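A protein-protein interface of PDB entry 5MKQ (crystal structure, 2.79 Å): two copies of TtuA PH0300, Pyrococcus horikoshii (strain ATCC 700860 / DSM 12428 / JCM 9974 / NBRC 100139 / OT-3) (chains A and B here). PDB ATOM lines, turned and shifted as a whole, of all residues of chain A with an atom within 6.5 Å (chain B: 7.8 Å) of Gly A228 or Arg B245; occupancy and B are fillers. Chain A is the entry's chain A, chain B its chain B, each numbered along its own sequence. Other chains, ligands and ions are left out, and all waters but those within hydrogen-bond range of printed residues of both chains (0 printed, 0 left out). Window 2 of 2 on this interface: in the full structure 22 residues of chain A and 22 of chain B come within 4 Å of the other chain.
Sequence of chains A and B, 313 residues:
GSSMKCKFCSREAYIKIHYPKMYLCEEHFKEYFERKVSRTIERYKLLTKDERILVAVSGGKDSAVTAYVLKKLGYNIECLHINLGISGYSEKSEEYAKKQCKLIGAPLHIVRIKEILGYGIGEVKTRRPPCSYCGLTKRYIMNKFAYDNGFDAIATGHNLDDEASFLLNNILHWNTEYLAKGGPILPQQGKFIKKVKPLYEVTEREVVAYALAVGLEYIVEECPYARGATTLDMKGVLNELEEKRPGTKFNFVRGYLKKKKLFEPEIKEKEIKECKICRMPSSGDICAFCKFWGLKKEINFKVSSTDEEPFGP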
ATOM      1  N   HIS A 173      -9.138  -5.004 -30.054  1.00  0.00           N
ATOM      2  CA  HIS A 173      -8.314  -6.157 -29.684  1.00  0.00           C
ATOM      3  C   HIS A 173      -7.647  -6.806 -30.895  1.00  0.00           C
ATOM      4  O   HIS A 173      -6.932  -7.799 -30.739  1.00  0.00           O
ATOM      5  CB  HIS A 173      -9.138  -7.193 -28.909  1.00  0.00           C
ATOM      6  CG  HIS A 173      -9.632  -6.685 -27.597  1.00  0.00           C
ATOM      7  ND1 HIS A 173     -10.961  -6.364 -27.406  1.00  0.00           N
ATOM      8  CD2 HIS A 173      -8.948  -6.421 -26.463  1.00  0.00           C
ATOM      9  CE1 HIS A 173     -11.047  -5.924 -26.162  1.00  0.00           C
ATOM     10  NE2 HIS A 173      -9.861  -5.941 -25.556  1.00  0.00           N
ATOM     11  N   TYR A 225     -23.312 -13.274 -15.293  1.00  0.00           N
ATOM     12  CA  TYR A 225     -21.912 -13.495 -15.664  1.00  0.00           C
ATOM     13  C   TYR A 225     -21.515 -12.683 -16.899  1.00  0.00           C
ATOM     14  O   TYR A 225     -21.980 -11.558 -17.098  1.00  0.00           O
ATOM     15  CB  TYR A 225     -21.624 -14.991 -15.891  1.00  0.00           C
ATOM     16  CG  TYR A 225     -22.385 -15.926 -14.972  1.00  0.00           C
ATOM     17  CD1 TYR A 225     -23.501 -16.620 -15.425  1.00  0.00           C
ATOM     18  CD2 TYR A 225     -21.971 -16.138 -13.661  1.00  0.00           C
ATOM     19  CE1 TYR A 225     -24.199 -17.490 -14.591  1.00  0.00           C
ATOM     20  CE2 TYR A 225     -22.654 -17.016 -12.821  1.00  0.00           C
ATOM     21  CZ  TYR A 225     -23.771 -17.687 -13.290  1.00  0.00           C
ATOM     22  OH  TYR A 225     -24.458 -18.557 -12.478  1.00  0.00           O
ATOM     23  N   GLY A 228     -17.631  -7.268 -15.344  1.00  0.00           N
ATOM     24  CA  GLY A 228     -18.368  -6.308 -16.157  1.00  0.00           C
ATOM     25  C   GLY A 228     -18.300  -6.596 -17.644  1.00  0.00           C
ATOM     26  O   GLY A 228     -17.205  -6.788 -18.185  1.00  0.00           O
ATOM     27  N   ALA A 229     -19.473  -6.623 -18.317  1.00  0.00           N
ATOM     28  CA  ALA A 229     -19.577  -6.894 -19.755  1.00  0.00           C
ATOM     29  C   ALA A 229     -19.072  -5.729 -20.606  1.00  0.00           C
ATOM     30  O   ALA A 229     -19.505  -4.583 -20.433  1.00  0.00           O
ATOM     31  CB  ALA A 229     -21.005  -7.258 -20.136  1.00  0.00           C
ATOM     32  N   THR A 230     -18.138  -6.043 -21.522  1.00  0.00           N
ATOM     33  CA  THR A 230     -17.494  -5.103 -22.445  1.00  0.00           C
ATOM     34  C   THR A 230     -18.456  -4.572 -23.528  1.00  0.00           C
ATOM     35  O   THR A 230     -18.229  -3.484 -24.055  1.00  0.00           O
ATOM     36  CB  THR A 230     -16.207  -5.718 -23.038  1.00  0.00           C
ATOM     37  OG1 THR A 230     -15.518  -4.725 -23.798  1.00  0.00           O
ATOM     38  CG2 THR A 230     -16.463  -6.970 -23.894  1.00  0.00           C
ATOM     39  N   THR A 231     -19.517  -5.343 -23.851  1.00  0.00           N
ATOM     40  CA  THR A 231     -20.532  -5.015 -24.861  1.00  0.00           C
ATOM     41  C   THR A 231     -21.223  -3.677 -24.565  1.00  0.00           C
ATOM     42  O   THR A 231     -21.288  -2.827 -25.454  1.00  0.00           O
ATOM     43  CB  THR A 231     -21.544  -6.177 -25.018  1.00  0.00           C
ATOM     44  OG1 THR A 231     -20.848  -7.424 -25.088  1.00  0.00           O
ATOM     45  CG2 THR A 231     -22.439  -6.020 -26.245  1.00  0.00           C
ATOM     46  N   ASP A 233     -20.205  -1.209 -22.811  1.00  0.00           N
ATOM     47  CA  ASP A 233     -19.225  -0.129 -22.882  1.00  0.00           C
ATOM     48  C   ASP A 233     -19.148   0.389 -24.325  1.00  0.00           C
ATOM     49  O   ASP A 233     -19.304   1.593 -24.549  1.00  0.00           O
ATOM     50  CB  ASP A 233     -17.838  -0.609 -22.394  1.00  0.00           C
ATOM     51  CG  ASP A 233     -17.782  -1.047 -20.940  1.00  0.00           C
ATOM     52  OD1 ASP A 233     -17.968  -0.184 -20.048  1.00  0.00           O
ATOM     53  OD2 ASP A 233     -17.483  -2.236 -20.688  1.00  0.00           O
ATOM     54  N   MET A 234     -18.960  -0.535 -25.299  1.00  0.00           N
ATOM     55  CA  MET A 234     -18.859  -0.258 -26.739  1.00  0.00           C
ATOM     56  C   MET A 234     -20.116   0.414 -27.269  1.00  0.00           C
ATOM     57  O   MET A 234     -20.011   1.380 -28.024  1.00  0.00           O
ATOM     58  CB  MET A 234     -18.593  -1.547 -27.545  1.00  0.00           C
ATOM     59  CG  MET A 234     -17.380  -2.337 -27.095  1.00  0.00           C
ATOM     60  SD  MET A 234     -15.806  -1.507 -27.382  1.00  0.00           S
ATOM     61  CE  MET A 234     -14.829  -2.247 -26.095  1.00  0.00           C
ATOM     62  N   TYR B  19      -1.096   3.473 -15.713  1.00  0.00           N
ATOM     63  CA  TYR B  19      -0.568   2.191 -16.178  1.00  0.00           C
ATOM     64  C   TYR B  19       0.895   2.384 -16.687  1.00  0.00           C
ATOM     65  O   TYR B  19       1.098   3.050 -17.708  1.00  0.00           O
ATOM     66  CB  TYR B  19      -1.545   1.502 -17.188  1.00  0.00           C
ATOM     67  CG  TYR B  19      -0.938   1.004 -18.483  1.00  0.00           C
ATOM     68  CD1 TYR B  19      -0.192  -0.169 -18.522  1.00  0.00           C
ATOM     69  CD2 TYR B  19      -1.133   1.694 -19.676  1.00  0.00           C
ATOM     70  CE1 TYR B  19       0.395  -0.615 -19.706  1.00  0.00           C
ATOM     71  CE2 TYR B  19      -0.571   1.244 -20.872  1.00  0.00           C
ATOM     72  CZ  TYR B  19       0.183   0.083 -20.882  1.00  0.00           C
ATOM     73  OH  TYR B  19       0.738  -0.383 -22.048  1.00  0.00           O
ATOM     74  N   LEU B 238     -12.081   7.524 -26.323  1.00  0.00           N
ATOM     75  CA  LEU B 238     -10.958   6.669 -25.936  1.00  0.00           C
ATOM     76  C   LEU B 238     -10.543   6.870 -24.483  1.00  0.00           C
ATOM     77  O   LEU B 238     -10.048   5.929 -23.864  1.00  0.00           O
ATOM     78  CB  LEU B 238      -9.770   6.860 -26.883  1.00  0.00           C
ATOM     79  CG  LEU B 238      -9.956   6.281 -28.283  1.00  0.00           C
ATOM     80  CD1 LEU B 238      -9.181   7.066 -29.290  1.00  0.00           C
ATOM     81  CD2 LEU B 238      -9.571   4.802 -28.342  1.00  0.00           C
ATOM     82  N   ASN B 239     -10.756   8.082 -23.936  1.00  0.00           N
ATOM     83  CA  ASN B 239     -10.466   8.399 -22.536  1.00  0.00           C
ATOM     84  C   ASN B 239     -11.498   7.715 -21.647  1.00  0.00           C
ATOM     85  O   ASN B 239     -11.150   7.223 -20.576  1.00  0.00           O
ATOM     86  CB  ASN B 239     -10.471   9.909 -22.294  1.00  0.00           C
ATOM     87  CG  ASN B 239      -9.217  10.637 -22.724  1.00  0.00           C
ATOM     88  OD1 ASN B 239      -8.303  10.080 -23.346  1.00  0.00           O
ATOM     89  ND2 ASN B 239      -9.161  11.922 -22.414  1.00  0.00           N
ATOM     90  N   GLU B 240     -12.762   7.658 -22.118  1.00  0.00           N
ATOM     91  CA  GLU B 240     -13.879   6.990 -21.443  1.00  0.00           C
ATOM     92  C   GLU B 240     -13.580   5.481 -21.350  1.00  0.00           C
ATOM     93  O   GLU B 240     -13.786   4.876 -20.292  1.00  0.00           O
ATOM     94  CB  GLU B 240     -15.192   7.237 -22.210  1.00  0.00           C
ATOM     95  CG  GLU B 240     -16.454   6.997 -21.390  1.00  0.00           C
ATOM     96  CD  GLU B 240     -17.731   6.735 -22.173  1.00  0.00           C
ATOM     97  OE1 GLU B 240     -17.856   7.239 -23.314  1.00  0.00           O
ATOM     98  OE2 GLU B 240     -18.622   6.040 -21.632  1.00  0.00           O
ATOM     99  N   LEU B 241     -13.060   4.897 -22.452  1.00  0.00           N
ATOM    100  CA  LEU B 241     -12.674   3.487 -22.547  1.00  0.00           C
ATOM    101  C   LEU B 241     -11.477   3.165 -21.650  1.00  0.00           C
ATOM    102  O   LEU B 241     -11.454   2.103 -21.027  1.00  0.00           O
ATOM    103  CB  LEU B 241     -12.367   3.101 -24.007  1.00  0.00           C
ATOM    104  CG  LEU B 241     -13.569   2.978 -24.953  1.00  0.00           C
ATOM    105  CD1 LEU B 241     -13.161   3.216 -26.385  1.00  0.00           C
ATOM    106  CD2 LEU B 241     -14.238   1.628 -24.822  1.00  0.00           C
ATOM    107  N   GLU B 242     -10.497   4.089 -21.577  1.00  0.00           N
ATOM    108  CA  GLU B 242      -9.285   3.951 -20.761  1.00  0.00           C
ATOM    109  C   GLU B 242      -9.591   3.908 -19.257  1.00  0.00           C
ATOM    110  O   GLU B 242      -8.894   3.199 -18.524  1.00  0.00           O
ATOM    111  CB  GLU B 242      -8.269   5.061 -21.096  1.00  0.00           C
ATOM    112  CG  GLU B 242      -6.831   4.748 -20.707  1.00  0.00           C
ATOM    113  CD  GLU B 242      -6.105   3.737 -21.576  1.00  0.00           C
ATOM    114  OE1 GLU B 242      -5.115   4.124 -22.236  1.00  0.00           O
ATOM    115  OE2 GLU B 242      -6.497   2.548 -21.564  1.00  0.00           O
ATOM    116  N   GLU B 243     -10.635   4.652 -18.808  1.00  0.00           N
ATOM    117  CA  GLU B 243     -11.104   4.704 -17.416  1.00  0.00           C
ATOM    118  C   GLU B 243     -11.489   3.302 -16.939  1.00  0.00           C
ATOM    119  O   GLU B 243     -10.934   2.813 -15.956  1.00  0.00           O
ATOM    120  CB  GLU B 243     -12.328   5.630 -17.285  1.00  0.00           C
ATOM    121  CG  GLU B 243     -12.019   7.116 -17.316  1.00  0.00           C
ATOM    122  CD  GLU B 243     -13.247   8.006 -17.256  1.00  0.00           C
ATOM    123  OE1 GLU B 243     -13.577   8.629 -18.290  1.00  0.00           O
ATOM    124  OE2 GLU B 243     -13.888   8.072 -16.180  1.00  0.00           O
ATOM    125  N   LYS B 244     -12.417   2.653 -17.667  1.00  0.00           N
ATOM    126  CA  LYS B 244     -12.911   1.311 -17.377  1.00  0.00           C
ATOM    127  C   LYS B 244     -11.808   0.266 -17.566  1.00  0.00           C
ATOM    128  O   LYS B 244     -11.469  -0.444 -16.617  1.00  0.00           O
ATOM    129  CB  LYS B 244     -14.139   0.990 -18.248  1.00  0.00           C
ATOM    130  CG  LYS B 244     -15.378   1.789 -17.873  1.00  0.00           C
ATOM    131  CD  LYS B 244     -16.015   2.438 -19.087  1.00  0.00           C
ATOM    132  CE  LYS B 244     -17.263   3.197 -18.725  1.00  0.00           C
ATOM    133  NZ  LYS B 244     -17.900   3.803 -19.923  1.00  0.00           N
ATOM    134  N   ARG B 245     -11.226   0.205 -18.778  1.00  0.00           N
ATOM    135  CA  ARG B 245     -10.165  -0.735 -19.121  1.00  0.00           C
ATOM    136  C   ARG B 245      -8.836  -0.008 -19.361  1.00  0.00           C
ATOM    137  O   ARG B 245      -8.646   0.572 -20.431  1.00  0.00           O
ATOM    138  CB  ARG B 245     -10.569  -1.600 -20.332  1.00  0.00           C
ATOM    139  CG  ARG B 245     -10.719  -3.085 -20.008  1.00  0.00           C
ATOM    140  CD  ARG B 245     -11.819  -3.755 -20.825  1.00  0.00           C
ATOM    141  NE  ARG B 245     -13.157  -3.336 -20.396  1.00  0.00           N
ATOM    142  CZ  ARG B 245     -14.134  -4.162 -20.031  1.00  0.00           C
ATOM    143  NH1 ARG B 245     -13.949  -5.478 -20.060  1.00  0.00           N
ATOM    144  NH2 ARG B 245     -15.308  -3.680 -19.650  1.00  0.00           N
ATOM    145  N   PRO B 246      -7.904  -0.003 -18.377  1.00  0.00           N
ATOM    146  CA  PRO B 246      -6.609   0.674 -18.595  1.00  0.00           C
ATOM    147  C   PRO B 246      -5.702  -0.126 -19.533  1.00  0.00           C
ATOM    148  O   PRO B 246      -5.756  -1.357 -19.552  1.00  0.00           O
ATOM    149  CB  PRO B 246      -6.019   0.811 -17.179  1.00  0.00           C
ATOM    150  CG  PRO B 246      -7.110   0.326 -16.234  1.00  0.00           C
ATOM    151  CD  PRO B 246      -7.961  -0.609 -17.035  1.00  0.00           C
ATOM    152  N   GLY B 247      -4.907   0.591 -20.324  1.00  0.00           N
ATOM    153  CA  GLY B 247      -4.000   0.007 -21.308  1.00  0.00           C
ATOM    154  C   GLY B 247      -4.591  -0.116 -22.705  1.00  0.00           C
ATOM    155  O   GLY B 247      -3.861  -0.419 -23.657  1.00  0.00           O
ATOM    156  N   THR B 248      -5.925   0.119 -22.830  1.00  0.00           N
ATOM    157  CA  THR B 248      -6.719   0.076 -24.066  1.00  0.00           C
ATOM    158  C   THR B 248      -6.012   0.788 -25.221  1.00  0.00           C
ATOM    159  O   THR B 248      -5.726   0.142 -26.228  1.00  0.00           O
ATOM    160  CB  THR B 248      -8.140   0.599 -23.798  1.00  0.00           C
ATOM    161  OG1 THR B 248      -8.807  -0.336 -22.960  1.00  0.00           O
ATOM    162  CG2 THR B 248      -8.959   0.802 -25.070  1.00  0.00           C
ATOM    163  N   LYS B 249      -5.700   2.094 -25.054  1.00  0.00           N
ATOM    164  CA  LYS B 249      -5.021   2.915 -26.057  1.00  0.00           C
ATOM    165  C   LYS B 249      -3.757   2.236 -26.580  1.00  0.00           C
ATOM    166  O   LYS B 249      -3.603   2.105 -27.793  1.00  0.00           O
ATOM    167  CB  LYS B 249      -4.660   4.293 -25.485  1.00  0.00           C
ATOM    168  CG  LYS B 249      -5.810   5.273 -25.372  1.00  0.00           C
ATOM    169  CD  LYS B 249      -5.311   6.562 -24.733  1.00  0.00           C
ATOM    170  CE  LYS B 249      -6.428   7.484 -24.325  1.00  0.00           C
ATOM    171  NZ  LYS B 249      -5.929   8.604 -23.485  1.00  0.00           N
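The side-chain carboxylate (OD1) of Asp A233 lies within salt-bridge range of the side-chain amino group (NZ) of Lys B244 (3.99 Å).
The side-chain carboxylate (OD2) of Asp A233 lies within salt-bridge range of the guanidinium group (NH2) of Arg B245, at 2.8 Å.
The backbone carbonyl oxygen of Arg B245 lies within hydrogen-bond range of the side-chain hydroxyl of Thr B248, 2.7 Å away.
The side-chain carboxylate (OE2) of Glu B240 lies within salt-bridge range of the side-chain amino group (NZ) of Lys B244.
Among the printed residues, pairs that only touch across the chains: Thr A230 with Arg B245 (3.7 Å) and Gly A228 with Arg B245 (3.9 Å).
Gly A228 touches just one residue of chain B: Arg B245 (3.9 Å).
Arg B245 touches three residues of chain A.
No residue of chain B comes within 4 Å of Ala A229.
Of the printed residues of chain B, Asp A233 touches Lys B244 and Arg B245.
Of the printed residues of chain B, Thr A230 touches Arg B245 (3.7 Å).
Printed residues of chain A within 4 Å of Lys B244: Asp A233.
Thr B248 touches none of the printed residues of chain A.
The nearest printed residue of chain B that does not touch Gly A228 is Lys B244 (8.4 Å).
The nearest residue of chain A that does not touch Arg B245 is Ala A229 (4.4 Å).
Of the 8 printed residues of chain A, 3 touch a printed residue of chain B.
Printed residues of chain A that touch a printed residue of chain B: Gly A228, Thr A230 and Asp A233.
Along chain A the printed residues that touch a printed residue of chain B span positions 228 to 233.
No position is printed for both chains.
Of the 4 pairs that touch across the chains among the printed residues, none has its exchanged pair printed and touching as well.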
